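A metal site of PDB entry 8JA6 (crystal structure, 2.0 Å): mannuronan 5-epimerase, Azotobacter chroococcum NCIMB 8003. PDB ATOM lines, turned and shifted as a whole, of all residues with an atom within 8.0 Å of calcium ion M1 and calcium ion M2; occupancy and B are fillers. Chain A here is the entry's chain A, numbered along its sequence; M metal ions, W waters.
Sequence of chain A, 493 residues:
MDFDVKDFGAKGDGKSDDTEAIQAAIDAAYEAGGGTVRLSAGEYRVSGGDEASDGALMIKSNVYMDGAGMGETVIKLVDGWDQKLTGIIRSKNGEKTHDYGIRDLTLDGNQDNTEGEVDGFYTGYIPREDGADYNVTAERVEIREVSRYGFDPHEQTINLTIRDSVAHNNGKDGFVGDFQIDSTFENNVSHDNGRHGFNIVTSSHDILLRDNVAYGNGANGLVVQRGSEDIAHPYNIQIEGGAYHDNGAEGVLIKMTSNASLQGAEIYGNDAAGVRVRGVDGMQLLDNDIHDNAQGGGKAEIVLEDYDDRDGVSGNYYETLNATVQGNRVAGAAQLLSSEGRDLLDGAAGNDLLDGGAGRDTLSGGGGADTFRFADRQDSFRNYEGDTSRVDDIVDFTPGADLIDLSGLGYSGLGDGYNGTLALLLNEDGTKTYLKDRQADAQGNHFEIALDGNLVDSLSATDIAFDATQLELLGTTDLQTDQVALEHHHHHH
N of Gly 365 lies within hydrogen-bond range of OD1 of Asp 396 (2.9 Å). The backbone carbonyl oxygen (O) of Asp 370 is in hydrogen-bond range of the backbone NH (N) of Leu 403 (2.8 Å). The side-chain carboxylate (OD1) of Asp 352 sits at hydrogen-bond distance from the backbone NH (N) of Ala 334, at 2.8 Å. N of Thr 371 is in hydrogen-bond range of O of Asp 352, at 2.8 Å. The backbone NH (N) of Gly 366 lies within hydrogen-bond range of the side-chain carboxylate (OD2) of Asp 396, at 2.8 Å. OD2 of Asp 402 is in hydrogen-bond range of N of Thr 398 (2.8 Å).
Of the 29 residues printed, 5 come within 4 Å of calcium ion M1. Along chain A the residues within 4 Å of calcium ion M1 span positions 366 to 402.
Within 4 Å of calcium ion M2: Ala 348, Gly 350, Asp 352, Gly 365, Gly 366, Gly 367 and Asp 370.
Calcium ion M1 is bound by the side-chain carboxylate (OD1) of Asp 370 (2.3 Å), the backbone carbonyl oxygen (O) of Gly 366 (2.4 Å), the backbone carbonyl oxygen (O) of Gly 368 (2.5 Å), water W2 (2.5 Å), the side-chain carboxylate (OD1) of Asp 402 (2.6 Å) and water W1 (2.6 Å). Calcium ion M1 has six donor atoms within binding distance.
Calcium ion M2 is bound by O of Gly 365 (2.3 Å), O of Ala 348 (2.3 Å), OD2 of Asp 370 (2.3 Å), OD2 of Asp 352 (2.4 Å), O of Gly 350 (2.4 Å), O of Gly 367 (2.4 Å) and OD1 of Asp 370 (2.9 Å).
Water W1 lies within hydrogen-bond range of the side-chain carboxylate (OD2) of Asp 402 (2.5 Å) and the backbone carbonyl oxygen (O) of Asp 396 (3.1 Å).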
ATOM      1  N   VAL A 330      34.764 -13.464   1.389  1.00  0.00           N
ATOM      2  CA  VAL A 330      33.783 -13.152   0.359  1.00  0.00           C
ATOM      3  C   VAL A 330      33.102 -11.846   0.738  1.00  0.00           C
ATOM      4  O   VAL A 330      32.303 -11.812   1.678  1.00  0.00           O
ATOM      5  CB  VAL A 330      32.718 -14.249   0.206  1.00  0.00           C
ATOM      6  CG1 VAL A 330      31.898 -14.039  -1.073  1.00  0.00           C
ATOM      7  CG2 VAL A 330      33.355 -15.646   0.229  1.00  0.00           C
ATOM      8  N   GLY A 332      30.511 -10.045  -0.081  1.00  0.00           N
ATOM      9  CA  GLY A 332      29.226 -10.045  -0.767  1.00  0.00           C
ATOM     10  C   GLY A 332      28.515 -11.357  -0.522  1.00  0.00           C
ATOM     11  O   GLY A 332      28.989 -12.223   0.209  1.00  0.00           O
ATOM     12  N   ALA A 333      27.362 -11.494  -1.172  1.00  0.00           N
ATOM     13  CA  ALA A 333      26.465 -12.605  -0.878  1.00  0.00           C
ATOM     14  C   ALA A 333      26.928 -13.910  -1.513  1.00  0.00           C
ATOM     15  O   ALA A 333      27.328 -13.948  -2.687  1.00  0.00           O
ATOM     16  CB  ALA A 333      25.050 -12.295  -1.370  1.00  0.00           C
ATOM     17  N   ALA A 334      26.831 -14.985  -0.745  1.00  0.00           N
ATOM     18  CA  ALA A 334      27.061 -16.338  -1.251  1.00  0.00           C
ATOM     19  C   ALA A 334      25.746 -17.111  -1.265  1.00  0.00           C
ATOM     20  O   ALA A 334      25.027 -17.152  -0.260  1.00  0.00           O
ATOM     21  CB  ALA A 334      28.109 -17.069  -0.394  1.00  0.00           C
ATOM     22  N   ASP A 346      29.794 -23.003   4.515  1.00  0.00           N
ATOM     23  CA  ASP A 346      30.146 -21.871   5.362  1.00  0.00           C
ATOM     24  C   ASP A 346      29.999 -20.591   4.550  1.00  0.00           C
ATOM     25  O   ASP A 346      30.671 -20.434   3.514  1.00  0.00           O
ATOM     26  CB  ASP A 346      31.578 -21.985   5.891  1.00  0.00           C
ATOM     27  CG  ASP A 346      31.782 -23.175   6.834  1.00  0.00           C
ATOM     28  OD1 ASP A 346      32.960 -23.539   7.059  1.00  0.00           O
ATOM     29  OD2 ASP A 346      30.795 -23.730   7.363  1.00  0.00           O
ATOM     30  N   GLY A 347      29.137 -19.686   5.000  1.00  0.00           N
ATOM     31  CA  GLY A 347      29.089 -18.360   4.436  1.00  0.00           C
ATOM     32  C   GLY A 347      30.260 -17.513   4.923  1.00  0.00           C
ATOM     33  O   GLY A 347      31.155 -17.980   5.627  1.00  0.00           O
ATOM     34  N   ALA A 348      30.236 -16.241   4.548  1.00  0.00           N
ATOM     35  CA  ALA A 348      31.326 -15.306   4.834  1.00  0.00           C
ATOM     36  C   ALA A 348      30.679 -13.992   5.277  1.00  0.00           C
ATOM     37  O   ALA A 348      29.578 -13.987   5.832  1.00  0.00           O
ATOM     38  CB  ALA A 348      32.273 -15.183   3.632  1.00  0.00           C
ATOM     39  N   ALA A 349      31.407 -12.881   5.119  1.00  0.00           N
ATOM     40  CA  ALA A 349      30.969 -11.592   5.664  1.00  0.00           C
ATOM     41  C   ALA A 349      29.665 -11.093   5.056  1.00  0.00           C
ATOM     42  O   ALA A 349      29.057 -10.173   5.621  1.00  0.00           O
ATOM     43  CB  ALA A 349      32.056 -10.530   5.465  1.00  0.00           C
ATOM     44  N   GLY A 350      29.196 -11.653   3.929  1.00  0.00           N
ATOM     45  CA  GLY A 350      27.993 -11.165   3.283  1.00  0.00           C
ATOM     46  C   GLY A 350      26.713 -11.762   3.874  1.00  0.00           C
ATOM     47  O   GLY A 350      26.735 -12.557   4.804  1.00  0.00           O
ATOM     48  N   ASN A 351      25.583 -11.325   3.312  1.00  0.00           N
ATOM     49  CA  ASN A 351      24.266 -11.823   3.710  1.00  0.00           C
ATOM     50  C   ASN A 351      23.988 -13.027   2.814  1.00  0.00           C
ATOM     51  O   ASN A 351      23.604 -12.860   1.653  1.00  0.00           O
ATOM     52  CB  ASN A 351      23.177 -10.764   3.560  1.00  0.00           C
ATOM     53  CG  ASN A 351      23.340  -9.594   4.540  1.00  0.00           C
ATOM     54  OD1 ASN A 351      24.161  -9.616   5.451  1.00  0.00           O
ATOM     55  ND2 ASN A 351      22.535  -8.558   4.330  1.00  0.00           N
ATOM     56  N   ASP A 352      24.184 -14.220   3.338  1.00  0.00           N
ATOM     57  CA  ASP A 352      24.224 -15.423   2.524  1.00  0.00           C
ATOM     58  C   ASP A 352      22.942 -16.230   2.627  1.00  0.00           C
ATOM     59  O   ASP A 352      22.165 -16.083   3.574  1.00  0.00           O
ATOM     60  CB  ASP A 352      25.427 -16.301   2.921  1.00  0.00           C
ATOM     61  CG  ASP A 352      26.738 -15.506   3.005  1.00  0.00           C
ATOM     62  OD1 ASP A 352      27.069 -14.784   2.037  1.00  0.00           O
ATOM     63  OD2 ASP A 352      27.440 -15.617   4.032  1.00  0.00           O
ATOM     64  N   LEU A 353      22.727 -17.081   1.629  1.00  0.00           N
ATOM     65  CA  LEU A 353      21.614 -18.027   1.613  1.00  0.00           C
ATOM     66  C   LEU A 353      22.207 -19.433   1.642  1.00  0.00           C
ATOM     67  O   LEU A 353      23.021 -19.774   0.788  1.00  0.00           O
ATOM     68  CB  LEU A 353      20.746 -17.837   0.362  1.00  0.00           C
ATOM     69  CG  LEU A 353      19.679 -18.903   0.164  1.00  0.00           C
ATOM     70  CD1 LEU A 353      18.699 -18.806   1.327  1.00  0.00           C
ATOM     71  CD2 LEU A 353      18.964 -18.740  -1.179  1.00  0.00           C
ATOM     72  N   LEU A 354      21.821 -20.228   2.635  1.00  0.00           N
ATOM     73  CA  LEU A 354      22.374 -21.570   2.807  1.00  0.00           C
ATOM     74  C   LEU A 354      21.265 -22.611   2.833  1.00  0.00           C
ATOM     75  O   LEU A 354      20.310 -22.477   3.598  1.00  0.00           O
ATOM     76  CB  LEU A 354      23.189 -21.651   4.106  1.00  0.00           C
ATOM     77  CG  LEU A 354      24.395 -20.721   4.098  1.00  0.00           C
ATOM     78  CD1 LEU A 354      24.060 -19.469   4.862  1.00  0.00           C
ATOM     79  CD2 LEU A 354      25.608 -21.423   4.668  1.00  0.00           C
ATOM     80  N   SER A 364      27.075 -22.836   8.326  1.00  0.00           N
ATOM     81  CA  SER A 364      27.430 -21.678   9.122  1.00  0.00           C
ATOM     82  C   SER A 364      27.303 -20.422   8.269  1.00  0.00           C
ATOM     83  O   SER A 364      27.566 -20.439   7.067  1.00  0.00           O
ATOM     84  CB  SER A 364      28.834 -21.819   9.716  1.00  0.00           C
ATOM     85  OG  SER A 364      29.809 -21.475   8.770  1.00  0.00           O
ATOM     86  N   GLY A 365      26.853 -19.332   8.878  1.00  0.00           N
ATOM     87  CA  GLY A 365      26.655 -18.129   8.111  1.00  0.00           C
ATOM     88  C   GLY A 365      27.828 -17.161   8.107  1.00  0.00           C
ATOM     89  O   GLY A 365      27.996 -16.371   7.170  1.00  0.00           O
ATOM     90  N   GLY A 366      28.633 -17.191   9.167  1.00  0.00           N
ATOM     91  CA  GLY A 366      29.634 -16.144   9.286  1.00  0.00           C
ATOM     92  C   GLY A 366      29.003 -14.804   9.657  1.00  0.00           C
ATOM     93  O   GLY A 366      27.875 -14.722  10.184  1.00  0.00           O
ATOM     94  N   GLY A 367      29.747 -13.730   9.374  1.00  0.00           N
ATOM     95  CA  GLY A 367      29.264 -12.396   9.631  1.00  0.00           C
ATOM     96  C   GLY A 367      28.079 -12.058   8.747  1.00  0.00           C
ATOM     97  O   GLY A 367      27.723 -12.790   7.814  1.00  0.00           O
ATOM     98  N   GLY A 368      27.426 -10.941   9.056  1.00  0.00           N
ATOM     99  CA  GLY A 368      26.266 -10.521   8.302  1.00  0.00           C
ATOM    100  C   GLY A 368      25.009 -11.289   8.679  1.00  0.00           C
ATOM    101  O   GLY A 368      24.975 -12.095   9.608  1.00  0.00           O
ATOM    102  N   ALA A 369      23.932 -11.010   7.946  1.00  0.00           N
ATOM    103  CA  ALA A 369      22.611 -11.553   8.227  1.00  0.00           C
ATOM    104  C   ALA A 369      22.309 -12.641   7.208  1.00  0.00           C
ATOM    105  O   ALA A 369      22.069 -12.350   6.029  1.00  0.00           O
ATOM    106  CB  ALA A 369      21.559 -10.441   8.195  1.00  0.00           C
ATOM    107  N   ASP A 370      22.287 -13.888   7.664  1.00  0.00           N
ATOM    108  CA  ASP A 370      22.201 -15.039   6.771  1.00  0.00           C
ATOM    109  C   ASP A 370      20.881 -15.772   6.917  1.00  0.00           C
ATOM    110  O   ASP A 370      20.304 -15.822   8.006  1.00  0.00           O
ATOM    111  CB  ASP A 370      23.355 -16.002   7.038  1.00  0.00           C
ATOM    112  CG  ASP A 370      24.696 -15.307   6.974  1.00  0.00           C
ATOM    113  OD1 ASP A 370      25.363 -15.224   8.014  1.00  0.00           O
ATOM    114  OD2 ASP A 370      25.085 -14.840   5.877  1.00  0.00           O
ATOM    115  N   THR A 371      20.427 -16.363   5.814  1.00  0.00           N
ATOM    116  CA  THR A 371      19.195 -17.140   5.788  1.00  0.00           C
ATOM    117  C   THR A 371      19.558 -18.608   5.608  1.00  0.00           C
ATOM    118  O   THR A 371      20.246 -18.973   4.652  1.00  0.00           O
ATOM    119  CB  THR A 371      18.261 -16.656   4.670  1.00  0.00           C
ATOM    120  OG1 THR A 371      17.873 -15.295   4.942  1.00  0.00           O
ATOM    121  CG2 THR A 371      17.023 -17.489   4.613  1.00  0.00           C
ATOM    122  N   PHE A 372      19.128 -19.445   6.559  1.00  0.00           N
ATOM    123  CA  PHE A 372      19.301 -20.888   6.477  1.00  0.00           C
ATOM    124  C   PHE A 372      17.958 -21.472   6.072  1.00  0.00           C
ATOM    125  O   PHE A 372      17.007 -21.464   6.859  1.00  0.00           O
ATOM    126  CB  PHE A 372      19.757 -21.471   7.819  1.00  0.00           C
ATOM    127  CG  PHE A 372      21.011 -20.859   8.332  1.00  0.00           C
ATOM    128  CD1 PHE A 372      22.246 -21.427   8.013  1.00  0.00           C
ATOM    129  CD2 PHE A 372      20.986 -19.720   9.137  1.00  0.00           C
ATOM    130  CE1 PHE A 372      23.423 -20.849   8.484  1.00  0.00           C
ATOM    131  CE2 PHE A 372      22.151 -19.143   9.600  1.00  0.00           C
ATOM    132  CZ  PHE A 372      23.378 -19.716   9.295  1.00  0.00           C
ATOM    133  N   ASP A 396      26.443 -21.394  13.897  1.00  0.00           N
ATOM    134  CA  ASP A 396      26.640 -20.059  14.462  1.00  0.00           C
ATOM    135  C   ASP A 396      25.379 -19.213  14.327  1.00  0.00           C
ATOM    136  O   ASP A 396      25.464 -18.019  14.011  1.00  0.00           O
ATOM    137  CB  ASP A 396      27.809 -19.352  13.781  1.00  0.00           C
ATOM    138  CG  ASP A 396      27.560 -19.121  12.280  1.00  0.00           C
ATOM    139  OD1 ASP A 396      26.624 -19.736  11.714  1.00  0.00           O
ATOM    140  OD2 ASP A 396      28.287 -18.312  11.667  1.00  0.00           O
ATOM    141  N   PHE A 397      24.211 -19.798  14.546  1.00  0.00           N
ATOM    142  CA  PHE A 397      22.994 -19.020  14.382  1.00  0.00           C
ATOM    143  C   PHE A 397      22.973 -17.850  15.362  1.00  0.00           C
ATOM    144  O   PHE A 397      23.156 -18.027  16.566  1.00  0.00           O
ATOM    145  CB  PHE A 397      21.729 -19.859  14.587  1.00  0.00           C
ATOM    146  CG  PHE A 397      20.466 -19.126  14.183  1.00  0.00           C
ATOM    147  CD1 PHE A 397      19.725 -18.424  15.121  1.00  0.00           C
ATOM    148  CD2 PHE A 397      20.066 -19.083  12.860  1.00  0.00           C
ATOM    149  CE1 PHE A 397      18.591 -17.718  14.745  1.00  0.00           C
ATOM    150  CE2 PHE A 397      18.933 -18.377  12.485  1.00  0.00           C
ATOM    151  CZ  PHE A 397      18.193 -17.692  13.423  1.00  0.00           C
ATOM    152  N   THR A 398      22.728 -16.662  14.836  1.00  0.00           N
ATOM    153  CA  THR A 398      22.772 -15.419  15.615  1.00  0.00           C
ATOM    154  C   THR A 398      21.380 -14.814  15.691  1.00  0.00           C
ATOM    155  O   THR A 398      20.911 -14.206  14.702  1.00  0.00           O
ATOM    156  CB  THR A 398      23.770 -14.451  14.987  1.00  0.00           C
ATOM    157  OG1 THR A 398      24.992 -15.141  14.691  1.00  0.00           O
ATOM    158  CG2 THR A 398      24.063 -13.293  15.937  1.00  0.00           C
ATOM    159  N   ALA A 401      19.850 -11.419  13.976  1.00  0.00           N
ATOM    160  CA  ALA A 401      20.540 -11.168  12.713  1.00  0.00           C
ATOM    161  C   ALA A 401      20.235 -12.223  11.663  1.00  0.00           C
ATOM    162  O   ALA A 401      19.858 -11.878  10.533  1.00  0.00           O
ATOM    163  CB  ALA A 401      22.062 -11.073  12.954  1.00  0.00           C
ATOM    164  N   ASP A 402      20.404 -13.497  11.994  1.00  0.00           N
ATOM    165  CA  ASP A 402      20.139 -14.549  11.016  1.00  0.00           C
ATOM    166  C   ASP A 402      18.648 -14.905  10.973  1.00  0.00           C
ATOM    167  O   ASP A 402      17.845 -14.455  11.798  1.00  0.00           O
ATOM    168  CB  ASP A 402      20.966 -15.790  11.319  1.00  0.00           C
ATOM    169  CG  ASP A 402      22.459 -15.531  11.313  1.00  0.00           C
ATOM    170  OD1 ASP A 402      22.935 -14.666  10.524  1.00  0.00           O
ATOM    171  OD2 ASP A 402      23.155 -16.208  12.103  1.00  0.00           O
ATOM    172  N   LEU A 403      18.300 -15.738   9.997  1.00  0.00           N
ATOM    173  CA  LEU A 403      16.922 -16.153   9.799  1.00  0.00           C
ATOM    174  C   LEU A 403      16.902 -17.626   9.413  1.00  0.00           C
ATOM    175  O   LEU A 403      17.717 -18.073   8.609  1.00  0.00           O
ATOM    176  CB  LEU A 403      16.249 -15.311   8.693  1.00  0.00           C
ATOM    177  CG  LEU A 403      14.800 -15.709   8.349  1.00  0.00           C
ATOM    178  CD1 LEU A 403      13.814 -15.330   9.471  1.00  0.00           C
ATOM    179  CD2 LEU A 403      14.369 -15.094   7.013  1.00  0.00           C
ATOM    180  N   THR A 476      16.741 -12.010   4.824  1.00  0.00           N
ATOM    181  CA  THR A 476      17.956 -11.225   4.969  1.00  0.00           C
ATOM    182  C   THR A 476      18.713 -11.023   3.663  1.00  0.00           C
ATOM    183  O   THR A 476      19.621 -10.177   3.615  1.00  0.00           O
ATOM    184  CB  THR A 476      18.896 -11.873   5.993  1.00  0.00           C
ATOM    185  OG1 THR A 476      19.481 -13.057   5.431  1.00  0.00           O
ATOM    186  CG2 THR A 476      18.170 -12.219   7.282  1.00  0.00           C
HETATM  187 CA    CA M   1      25.466 -14.439  10.218  1.00  0.00          CA
HETATM  188 CA    CA M   2      27.363 -14.459   6.104  1.00  0.00          CA
HETATM  189  O   HOH W   1      25.382 -16.890  11.077  1.00  0.00           O
HETATM  190  O   HOH W   2      25.736 -13.342  12.420  1.00  0.00           O
